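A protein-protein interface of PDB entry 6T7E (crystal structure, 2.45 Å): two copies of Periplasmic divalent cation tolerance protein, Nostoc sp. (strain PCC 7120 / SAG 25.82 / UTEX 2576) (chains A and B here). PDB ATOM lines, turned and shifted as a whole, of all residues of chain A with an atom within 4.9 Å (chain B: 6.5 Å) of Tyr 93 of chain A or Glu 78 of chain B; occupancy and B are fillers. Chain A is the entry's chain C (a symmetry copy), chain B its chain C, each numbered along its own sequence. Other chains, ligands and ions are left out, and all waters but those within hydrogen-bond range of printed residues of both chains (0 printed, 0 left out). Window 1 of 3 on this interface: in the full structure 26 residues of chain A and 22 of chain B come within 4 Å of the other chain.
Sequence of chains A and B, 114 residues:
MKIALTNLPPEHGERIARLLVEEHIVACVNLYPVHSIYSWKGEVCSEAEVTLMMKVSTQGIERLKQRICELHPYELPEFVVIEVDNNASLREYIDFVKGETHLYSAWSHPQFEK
Among the printed residues, merely in contact across the chains: Met 53 of chain A with Leu 5 of chain B, Lys 55 of chain A with Asn 7 of chain B, Leu 90 of chain A with Pro 77 of chain B, Glu 92 of chain A with Leu 76 of chain B, Tyr 93 of chain A with Leu 76 of chain B, Tyr 93 of chain A with Pro 77 of chain B, Tyr 93 of chain A with Glu 78 of chain B, Tyr 93 of chain A with Val 80 of chain B and Phe 96 of chain A with Leu 76 of chain B.
Printed residues of chain B within 4 Å of Met 53 of chain A: Leu 5 (3.9 Å). Of the printed residues of chain B, Leu 90 of chain A touches Pro 77 and Phe 79. Tyr 93 of chain A touches just these residues of chain B: Leu 76 (3.7 Å), Pro 77 (3.6 Å), Glu 78 (3.6 Å) and Val 80 (3.6 Å). Ile 94 of chain A touches none of the printed residues of chain B. Printed residues of chain A within 4 Å of Leu 5 of chain B: Met 53. Of the printed residues of chain A, Glu 78 of chain B touches Lys 55 (2.6 Å) and Tyr 93 (3.6 Å). The nearest residue of chain B that does not touch Tyr 93 of chain A is Phe 79 of chain B (4.4 Å). The nearest residue of chain A that does not touch Glu 78 of chain B is Asn 30 of chain A (4.6 Å). The nearest printed residue of chain B that does not touch Lys 55 of chain A is Val 80 of chain B (5.2 Å).
No position is printed for both chains.
OE2 of Glu 78 of chain B is in salt-bridge range of NZ of Lys 55 of chain A (2.6 Å). The backbone carbonyl oxygen (O) of Phe 79 of chain B is in hydrogen-bond range of the backbone NH (N) of Leu 90 of chain A (3.1 Å). The side-chain amide nitrogen (ND2) of Asn 7 of chain B lies within hydrogen-bond range of the side-chain amide oxygen (OD1) of Asn 30 of chain A (2.9 Å).
Of the 13 printed residues of chain B, 7 touch a printed residue of chain A. Of the 13 printed residues of chain A, 7 touch a printed residue of chain B. Hydrophobic or aromatic side chains of chain A that line the printed part of chain B: Met 53, Leu 90, Tyr 93 and Phe 96.
The side-chain hydroxyl (OG1) of Thr 6 of chain B sits at hydrogen-bond distance from the backbone carbonyl oxygen (O) of Glu 78 of chain B (2.7 Å). O of Asn 30 of chain A sits at hydrogen-bond distance from N of Met 53 of chain A (2.8 Å). The side-chain amide nitrogen (ND2) of Asn 7 of chain B lies close to the side-chain carboxylate (OE1) of Glu 49 of chain B (3.2 Å). A ring nitrogen (NE2) of His 72 of chain B lies within hydrogen-bond range of the backbone carbonyl oxygen of Asn 7 of chain B (3.1 Å). The backbone NH of Lys 55 of chain A lies within hydrogen-bond range of the backbone carbonyl oxygen of Cys 28 of chain A (2.9 Å). OE1 of Glu 78 of chain B sits at hydrogen-bond distance from ND2 of Asn 7 of chain B, at 3.3 Å.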
ATOM      1  N   MET A   1      25.220  15.734   2.055  1.00  0.00           N
ATOM      2  CA  MET A   1      24.636  16.238   0.782  1.00  0.00           C
ATOM      3  C   MET A   1      23.538  17.260   1.041  1.00  0.00           C
ATOM      4  O   MET A   1      23.081  17.432   2.173  1.00  0.00           O
ATOM      5  CB  MET A   1      24.048  15.083  -0.027  1.00  0.00           C
ATOM      6  CG  MET A   1      22.883  14.389   0.663  1.00  0.00           C
ATOM      7  SD  MET A   1      21.910  13.331  -0.423  1.00  0.00           S
ATOM      8  CE  MET A   1      21.341  14.486  -1.670  1.00  0.00           C
ATOM      9  N   CYS A  28      23.606  13.656  -9.455  1.00  0.00           N
ATOM     10  CA  CYS A  28      22.359  13.220 -10.041  1.00  0.00           C
ATOM     11  C   CYS A  28      21.414  14.406 -10.205  1.00  0.00           C
ATOM     12  O   CYS A  28      21.460  15.370  -9.430  1.00  0.00           O
ATOM     13  CB  CYS A  28      21.711  12.155  -9.138  1.00  0.00           C
ATOM     14  SG  CYS A  28      20.052  11.648  -9.680  1.00  0.00           S
ATOM     15  N   ASN A  30      17.140  14.997 -11.162  1.00  0.00           N
ATOM     16  CA  ASN A  30      15.807  14.604 -11.585  1.00  0.00           C
ATOM     17  C   ASN A  30      15.111  15.794 -12.187  1.00  0.00           C
ATOM     18  O   ASN A  30      15.039  16.839 -11.565  1.00  0.00           O
ATOM     19  CB  ASN A  30      14.995  14.121 -10.400  1.00  0.00           C
ATOM     20  CG  ASN A  30      15.626  12.943  -9.719  1.00  0.00           C
ATOM     21  OD1 ASN A  30      15.546  12.805  -8.515  1.00  0.00           O
ATOM     22  ND2 ASN A  30      16.265  12.084 -10.493  1.00  0.00           N
ATOM     23  N   MET A  53      15.802  18.909  -9.866  1.00  0.00           N
ATOM     24  CA  MET A  53      16.096  18.569  -8.488  1.00  0.00           C
ATOM     25  C   MET A  53      17.470  17.904  -8.461  1.00  0.00           C
ATOM     26  O   MET A  53      17.646  16.757  -8.886  1.00  0.00           O
ATOM     27  CB  MET A  53      15.023  17.659  -7.902  1.00  0.00           C
ATOM     28  CG  MET A  53      15.157  17.474  -6.396  1.00  0.00           C
ATOM     29  SD  MET A  53      13.919  16.375  -5.673  1.00  0.00           S
ATOM     30  CE  MET A  53      14.719  14.779  -5.898  1.00  0.00           C
ATOM     31  N   LYS A  55      21.165  16.689  -6.818  1.00  0.00           N
ATOM     32  CA  LYS A  55      21.834  16.116  -5.652  1.00  0.00           C
ATOM     33  C   LYS A  55      23.309  16.442  -5.698  1.00  0.00           C
ATOM     34  O   LYS A  55      24.005  16.099  -6.652  1.00  0.00           O
ATOM     35  CB  LYS A  55      21.647  14.606  -5.590  1.00  0.00           C
ATOM     36  CG  LYS A  55      20.303  14.183  -5.054  1.00  0.00           C
ATOM     37  CD  LYS A  55      19.347  13.838  -6.165  1.00  0.00           C
ATOM     38  CE  LYS A  55      17.948  13.620  -5.616  1.00  0.00           C
ATOM     39  NZ  LYS A  55      17.170  12.685  -6.469  1.00  0.00           N
ATOM     40  N   LEU A  90      20.099   7.593   3.904  1.00  0.00           N
ATOM     41  CA  LEU A  90      20.951   6.413   3.782  1.00  0.00           C
ATOM     42  C   LEU A  90      22.413   6.800   3.555  1.00  0.00           C
ATOM     43  O   LEU A  90      22.745   7.504   2.599  1.00  0.00           O
ATOM     44  CB  LEU A  90      20.468   5.517   2.639  1.00  0.00           C
ATOM     45  CG  LEU A  90      21.194   4.163   2.530  1.00  0.00           C
ATOM     46  CD1 LEU A  90      20.911   3.287   3.747  1.00  0.00           C
ATOM     47  CD2 LEU A  90      20.813   3.442   1.233  1.00  0.00           C
ATOM     48  N   ARG A  91      23.279   6.312   4.433  1.00  0.00           N
ATOM     49  CA  ARG A  91      24.694   6.670   4.417  1.00  0.00           C
ATOM     50  C   ARG A  91      25.312   6.422   3.030  1.00  0.00           C
ATOM     51  O   ARG A  91      25.936   7.314   2.457  1.00  0.00           O
ATOM     52  CB  ARG A  91      25.451   5.890   5.503  1.00  0.00           C
ATOM     53  CG  ARG A  91      26.522   6.672   6.260  1.00  0.00           C
ATOM     54  CD  ARG A  91      27.553   7.329   5.358  1.00  0.00           C
ATOM     55  NE  ARG A  91      28.903   7.234   5.915  1.00  0.00           N
ATOM     56  N   GLU A  92      25.118   5.229   2.479  1.00  0.00           N
ATOM     57  CA  GLU A  92      25.776   4.884   1.214  1.00  0.00           C
ATOM     58  C   GLU A  92      25.320   5.757   0.038  1.00  0.00           C
ATOM     59  O   GLU A  92      26.104   6.030  -0.875  1.00  0.00           O
ATOM     60  CB  GLU A  92      25.692   3.377   0.871  1.00  0.00           C
ATOM     61  CG  GLU A  92      24.463   2.618   1.355  1.00  0.00           C
ATOM     62  CD  GLU A  92      24.632   2.047   2.758  1.00  0.00           C
ATOM     63  OE1 GLU A  92      25.349   1.041   2.894  1.00  0.00           O
ATOM     64  OE2 GLU A  92      24.049   2.598   3.724  1.00  0.00           O
ATOM     65  N   TYR A  93      24.067   6.216   0.067  1.00  0.00           N
ATOM     66  CA  TYR A  93      23.612   7.151  -0.946  1.00  0.00           C
ATOM     67  C   TYR A  93      24.327   8.489  -0.801  1.00  0.00           C
ATOM     68  O   TYR A  93      24.807   9.044  -1.785  1.00  0.00           O
ATOM     69  CB  TYR A  93      22.088   7.341  -0.940  1.00  0.00           C
ATOM     70  CG  TYR A  93      21.652   8.185  -2.123  1.00  0.00           C
ATOM     71  CD1 TYR A  93      21.730   7.684  -3.424  1.00  0.00           C
ATOM     72  CD2 TYR A  93      21.228   9.493  -1.957  1.00  0.00           C
ATOM     73  CE1 TYR A  93      21.370   8.454  -4.518  1.00  0.00           C
ATOM     74  CE2 TYR A  93      20.865  10.269  -3.048  1.00  0.00           C
ATOM     75  CZ  TYR A  93      20.940   9.745  -4.326  1.00  0.00           C
ATOM     76  OH  TYR A  93      20.587  10.515  -5.416  1.00  0.00           O
ATOM     77  N   ILE A  94      24.417   9.002   0.421  1.00  0.00           N
ATOM     78  CA  ILE A  94      25.135  10.260   0.663  1.00  0.00           C
ATOM     79  C   ILE A  94      26.579  10.139   0.190  1.00  0.00           C
ATOM     80  O   ILE A  94      27.107  11.043  -0.457  1.00  0.00           O
ATOM     81  CB  ILE A  94      25.126  10.648   2.156  1.00  0.00           C
ATOM     82  CG1 ILE A  94      23.708  11.017   2.590  1.00  0.00           C
ATOM     83  CG2 ILE A  94      26.082  11.806   2.439  1.00  0.00           C
ATOM     84  CD1 ILE A  94      23.583  11.251   4.079  1.00  0.00           C
ATOM     85  N   ASP A  95      27.212   9.022   0.530  1.00  0.00           N
ATOM     86  CA  ASP A  95      28.591   8.772   0.127  1.00  0.00           C
ATOM     87  C   ASP A  95      28.715   8.745  -1.391  1.00  0.00           C
ATOM     88  O   ASP A  95      29.640   9.332  -1.960  1.00  0.00           O
ATOM     89  CB  ASP A  95      29.109   7.454   0.720  1.00  0.00           C
ATOM     90  CG  ASP A  95      29.347   7.531   2.224  1.00  0.00           C
ATOM     91  OD1 ASP A  95      29.332   8.649   2.792  1.00  0.00           O
ATOM     92  OD2 ASP A  95      29.557   6.462   2.842  1.00  0.00           O
ATOM     93  N   PHE A  96      27.779   8.068  -2.042  1.00  0.00           N
ATOM     94  CA  PHE A  96      27.755   8.057  -3.488  1.00  0.00           C
ATOM     95  C   PHE A  96      27.665   9.488  -4.014  1.00  0.00           C
ATOM     96  O   PHE A  96      28.405   9.859  -4.925  1.00  0.00           O
ATOM     97  CB  PHE A  96      26.609   7.195  -4.019  1.00  0.00           C
ATOM     98  CG  PHE A  96      26.113   7.612  -5.381  1.00  0.00           C
ATOM     99  CD1 PHE A  96      26.824   7.282  -6.526  1.00  0.00           C
ATOM    100  CD2 PHE A  96      24.933   8.336  -5.515  1.00  0.00           C
ATOM    101  CE1 PHE A  96      26.367   7.665  -7.774  1.00  0.00           C
ATOM    102  CE2 PHE A  96      24.471   8.728  -6.762  1.00  0.00           C
ATOM    103  CZ  PHE A  96      25.186   8.384  -7.893  1.00  0.00           C
ATOM    104  N   VAL A  97      26.778  10.295  -3.436  1.00  0.00           N
ATOM    105  CA  VAL A  97      26.631  11.675  -3.877  1.00  0.00           C
ATOM    106  C   VAL A  97      27.912  12.467  -3.646  1.00  0.00           C
ATOM    107  O   VAL A  97      28.274  13.304  -4.471  1.00  0.00           O
ATOM    108  CB  VAL A  97      25.440  12.370  -3.197  1.00  0.00           C
ATOM    109  CG1 VAL A  97      25.478  13.877  -3.427  1.00  0.00           C
ATOM    110  CG2 VAL A  97      24.127  11.792  -3.714  1.00  0.00           C
ATOM    111  N   LEU B   5      12.473  10.901   0.294  1.00  0.00           N
ATOM    112  CA  LEU B   5      12.432  10.721  -1.147  1.00  0.00           C
ATOM    113  C   LEU B   5      13.177   9.482  -1.573  1.00  0.00           C
ATOM    114  O   LEU B   5      14.242   9.184  -1.048  1.00  0.00           O
ATOM    115  CB  LEU B   5      13.061  11.907  -1.852  1.00  0.00           C
ATOM    116  CG  LEU B   5      12.369  13.247  -1.666  1.00  0.00           C
ATOM    117  CD1 LEU B   5      13.220  14.306  -2.362  1.00  0.00           C
ATOM    118  CD2 LEU B   5      10.936  13.236  -2.202  1.00  0.00           C
ATOM    119  N   THR B   6      12.597   8.767  -2.527  1.00  0.00           N
ATOM    120  CA  THR B   6      13.328   7.783  -3.322  1.00  0.00           C
ATOM    121  C   THR B   6      12.877   7.839  -4.784  1.00  0.00           C
ATOM    122  O   THR B   6      11.868   8.459  -5.116  1.00  0.00           O
ATOM    123  CB  THR B   6      13.193   6.336  -2.789  1.00  0.00           C
ATOM    124  OG1 THR B   6      14.086   5.493  -3.514  1.00  0.00           O
ATOM    125  CG2 THR B   6      11.790   5.796  -2.952  1.00  0.00           C
ATOM    126  N   ASN B   7      13.661   7.197  -5.636  1.00  0.00           N
ATOM    127  CA  ASN B   7      13.364   7.054  -7.039  1.00  0.00           C
ATOM    128  C   ASN B   7      13.419   5.599  -7.366  1.00  0.00           C
ATOM    129  O   ASN B   7      14.322   4.914  -6.915  1.00  0.00           O
ATOM    130  CB  ASN B   7      14.408   7.769  -7.891  1.00  0.00           C
ATOM    131  CG  ASN B   7      14.177   9.260  -7.982  1.00  0.00           C
ATOM    132  OD1 ASN B   7      13.116   9.761  -7.655  1.00  0.00           O
ATOM    133  ND2 ASN B   7      15.181   9.976  -8.456  1.00  0.00           N
ATOM    134  N   GLU B  49      12.412   7.163 -14.380  1.00  0.00           N
ATOM    135  CA  GLU B  49      12.164   6.784 -13.002  1.00  0.00           C
ATOM    136  C   GLU B  49      10.898   7.453 -12.519  1.00  0.00           C
ATOM    137  O   GLU B  49      10.357   8.333 -13.173  1.00  0.00           O
ATOM    138  CB  GLU B  49      13.325   7.221 -12.112  1.00  0.00           C
ATOM    139  CG  GLU B  49      14.615   6.457 -12.362  1.00  0.00           C
ATOM    140  CD  GLU B  49      15.671   6.747 -11.317  1.00  0.00           C
ATOM    141  OE1 GLU B  49      15.697   7.881 -10.787  1.00  0.00           O
ATOM    142  OE2 GLU B  49      16.475   5.845 -11.021  1.00  0.00           O
ATOM    143  N   MET B  54       7.342  10.655   0.109  1.00  0.00           N
ATOM    144  CA  MET B  54       6.698   9.907   1.168  1.00  0.00           C
ATOM    145  C   MET B  54       6.543  10.722   2.439  1.00  0.00           C
ATOM    146  O   MET B  54       7.483  11.398   2.879  1.00  0.00           O
ATOM    147  CB  MET B  54       7.533   8.672   1.463  1.00  0.00           C
ATOM    148  CG  MET B  54       7.691   7.773   0.258  1.00  0.00           C
ATOM    149  SD  MET B  54       8.976   6.554   0.511  1.00  0.00           S
ATOM    150  CE  MET B  54      10.441   7.551   0.222  1.00  0.00           C
ATOM    151  N   ILE B  68      12.466   0.289   2.753  1.00  0.00           N
ATOM    152  CA  ILE B  68      12.946   0.736   1.456  1.00  0.00           C
ATOM    153  C   ILE B  68      14.171  -0.076   1.041  1.00  0.00           C
ATOM    154  O   ILE B  68      14.248  -0.529  -0.091  1.00  0.00           O
ATOM    155  CB  ILE B  68      13.280   2.245   1.464  1.00  0.00           C
ATOM    156  CG1 ILE B  68      11.998   3.078   1.535  1.00  0.00           C
ATOM    157  CG2 ILE B  68      14.094   2.645   0.235  1.00  0.00           C
ATOM    158  CD1 ILE B  68      11.152   3.057   0.284  1.00  0.00           C
ATOM    159  N   HIS B  72      13.676  -2.343  -2.360  1.00  0.00           N
ATOM    160  CA  HIS B  72      14.251  -1.621  -3.490  1.00  0.00           C
ATOM    161  C   HIS B  72      15.071  -2.534  -4.396  1.00  0.00           C
ATOM    162  O   HIS B  72      15.880  -3.307  -3.903  1.00  0.00           O
ATOM    163  CB  HIS B  72      15.148  -0.486  -2.986  1.00  0.00           C
ATOM    164  CG  HIS B  72      15.163   0.712  -3.875  1.00  0.00           C
ATOM    165  ND1 HIS B  72      15.851   0.745  -5.065  1.00  0.00           N
ATOM    166  CD2 HIS B  72      14.603   1.934  -3.728  1.00  0.00           C
ATOM    167  CE1 HIS B  72      15.708   1.934  -5.620  1.00  0.00           C
ATOM    168  NE2 HIS B  72      14.951   2.674  -4.830  1.00  0.00           N
ATOM    169  N   TYR B  74      17.395  -1.642  -6.707  1.00  0.00           N
ATOM    170  CA  TYR B  74      18.774  -1.179  -6.877  1.00  0.00           C
ATOM    171  C   TYR B  74      19.757  -1.661  -5.788  1.00  0.00           C
ATOM    172  O   TYR B  74      19.405  -1.805  -4.609  1.00  0.00           O
ATOM    173  CB  TYR B  74      18.820   0.356  -6.948  1.00  0.00           C
ATOM    174  CG  TYR B  74      18.073   1.005  -8.111  1.00  0.00           C
ATOM    175  CD1 TYR B  74      17.647   0.269  -9.221  1.00  0.00           C
ATOM    176  CD2 TYR B  74      17.834   2.382  -8.111  1.00  0.00           C
ATOM    177  CE1 TYR B  74      16.983   0.891 -10.272  1.00  0.00           C
ATOM    178  CE2 TYR B  74      17.167   3.006  -9.156  1.00  0.00           C
ATOM    179  CZ  TYR B  74      16.749   2.263 -10.232  1.00  0.00           C
ATOM    180  OH  TYR B  74      16.092   2.886 -11.271  1.00  0.00           O
ATOM    181  N   LEU B  76      22.361   0.123  -4.741  1.00  0.00           N
ATOM    182  CA  LEU B  76      22.495   1.290  -3.893  1.00  0.00           C
ATOM    183  C   LEU B  76      21.278   2.147  -4.152  1.00  0.00           C
ATOM    184  O   LEU B  76      21.205   2.830  -5.171  1.00  0.00           O
ATOM    185  CB  LEU B  76      23.780   2.046  -4.224  1.00  0.00           C
ATOM    186  CG  LEU B  76      24.223   3.133  -3.240  1.00  0.00           C
ATOM    187  CD1 LEU B  76      25.718   3.409  -3.367  1.00  0.00           C
ATOM    188  CD2 LEU B  76      23.429   4.410  -3.428  1.00  0.00           C
ATOM    189  N   PRO B  77      20.290   2.085  -3.254  1.00  0.00           N
ATOM    190  CA  PRO B  77      19.066   2.850  -3.472  1.00  0.00           C
ATOM    191  C   PRO B  77      19.168   4.293  -3.003  1.00  0.00           C
ATOM    192  O   PRO B  77      20.012   4.622  -2.173  1.00  0.00           O
ATOM    193  CB  PRO B  77      18.044   2.102  -2.629  1.00  0.00           C
ATOM    194  CG  PRO B  77      18.837   1.513  -1.523  1.00  0.00           C
ATOM    195  CD  PRO B  77      20.180   1.184  -2.098  1.00  0.00           C
ATOM    196  N   GLU B  78      18.308   5.142  -3.544  1.00  0.00           N
ATOM    197  CA  GLU B  78      18.151   6.490  -3.029  1.00  0.00           C
ATOM    198  C   GLU B  78      17.223   6.493  -1.801  1.00  0.00           C
ATOM    199  O   GLU B  78      16.110   5.981  -1.852  1.00  0.00           O
ATOM    200  CB  GLU B  78      17.584   7.401  -4.116  1.00  0.00           C
ATOM    201  CG  GLU B  78      17.347   8.825  -3.642  1.00  0.00           C
ATOM    202  CD  GLU B  78      17.160   9.806  -4.772  1.00  0.00           C
ATOM    203  OE1 GLU B  78      17.238   9.399  -5.960  1.00  0.00           O
ATOM    204  OE2 GLU B  78      16.933  10.990  -4.454  1.00  0.00           O
ATOM    205  N   PHE B  79      17.689   7.050  -0.691  1.00  0.00           N
ATOM    206  CA  PHE B  79      16.800   7.371   0.406  1.00  0.00           C
ATOM    207  C   PHE B  79      17.253   8.684   1.001  1.00  0.00           C
ATOM    208  O   PHE B  79      18.301   8.759   1.616  1.00  0.00           O
ATOM    209  CB  PHE B  79      16.764   6.274   1.466  1.00  0.00           C
ATOM    210  CG  PHE B  79      15.708   6.500   2.506  1.00  0.00           C
ATOM    211  CD1 PHE B  79      14.367   6.327   2.193  1.00  0.00           C
ATOM    212  CD2 PHE B  79      16.044   6.929   3.778  1.00  0.00           C
ATOM    213  CE1 PHE B  79      13.381   6.557   3.136  1.00  0.00           C
ATOM    214  CE2 PHE B  79      15.062   7.154   4.735  1.00  0.00           C
ATOM    215  CZ  PHE B  79      13.730   6.972   4.408  1.00  0.00           C
ATOM    216  N   VAL B  80      16.464   9.724   0.785  1.00  0.00           N
ATOM    217  CA  VAL B  80      16.847  11.055   1.197  1.00  0.00           C
ATOM    218  C   VAL B  80      15.752  11.639   2.047  1.00  0.00           C
ATOM    219  O   VAL B  80      14.607  11.707   1.610  1.00  0.00           O
ATOM    220  CB  VAL B  80      17.062  11.963  -0.016  1.00  0.00           C
ATOM    221  CG1 VAL B  80      17.358  13.396   0.432  1.00  0.00           C
ATOM    222  CG2 VAL B  80      18.193  11.417  -0.867  1.00  0.00           C
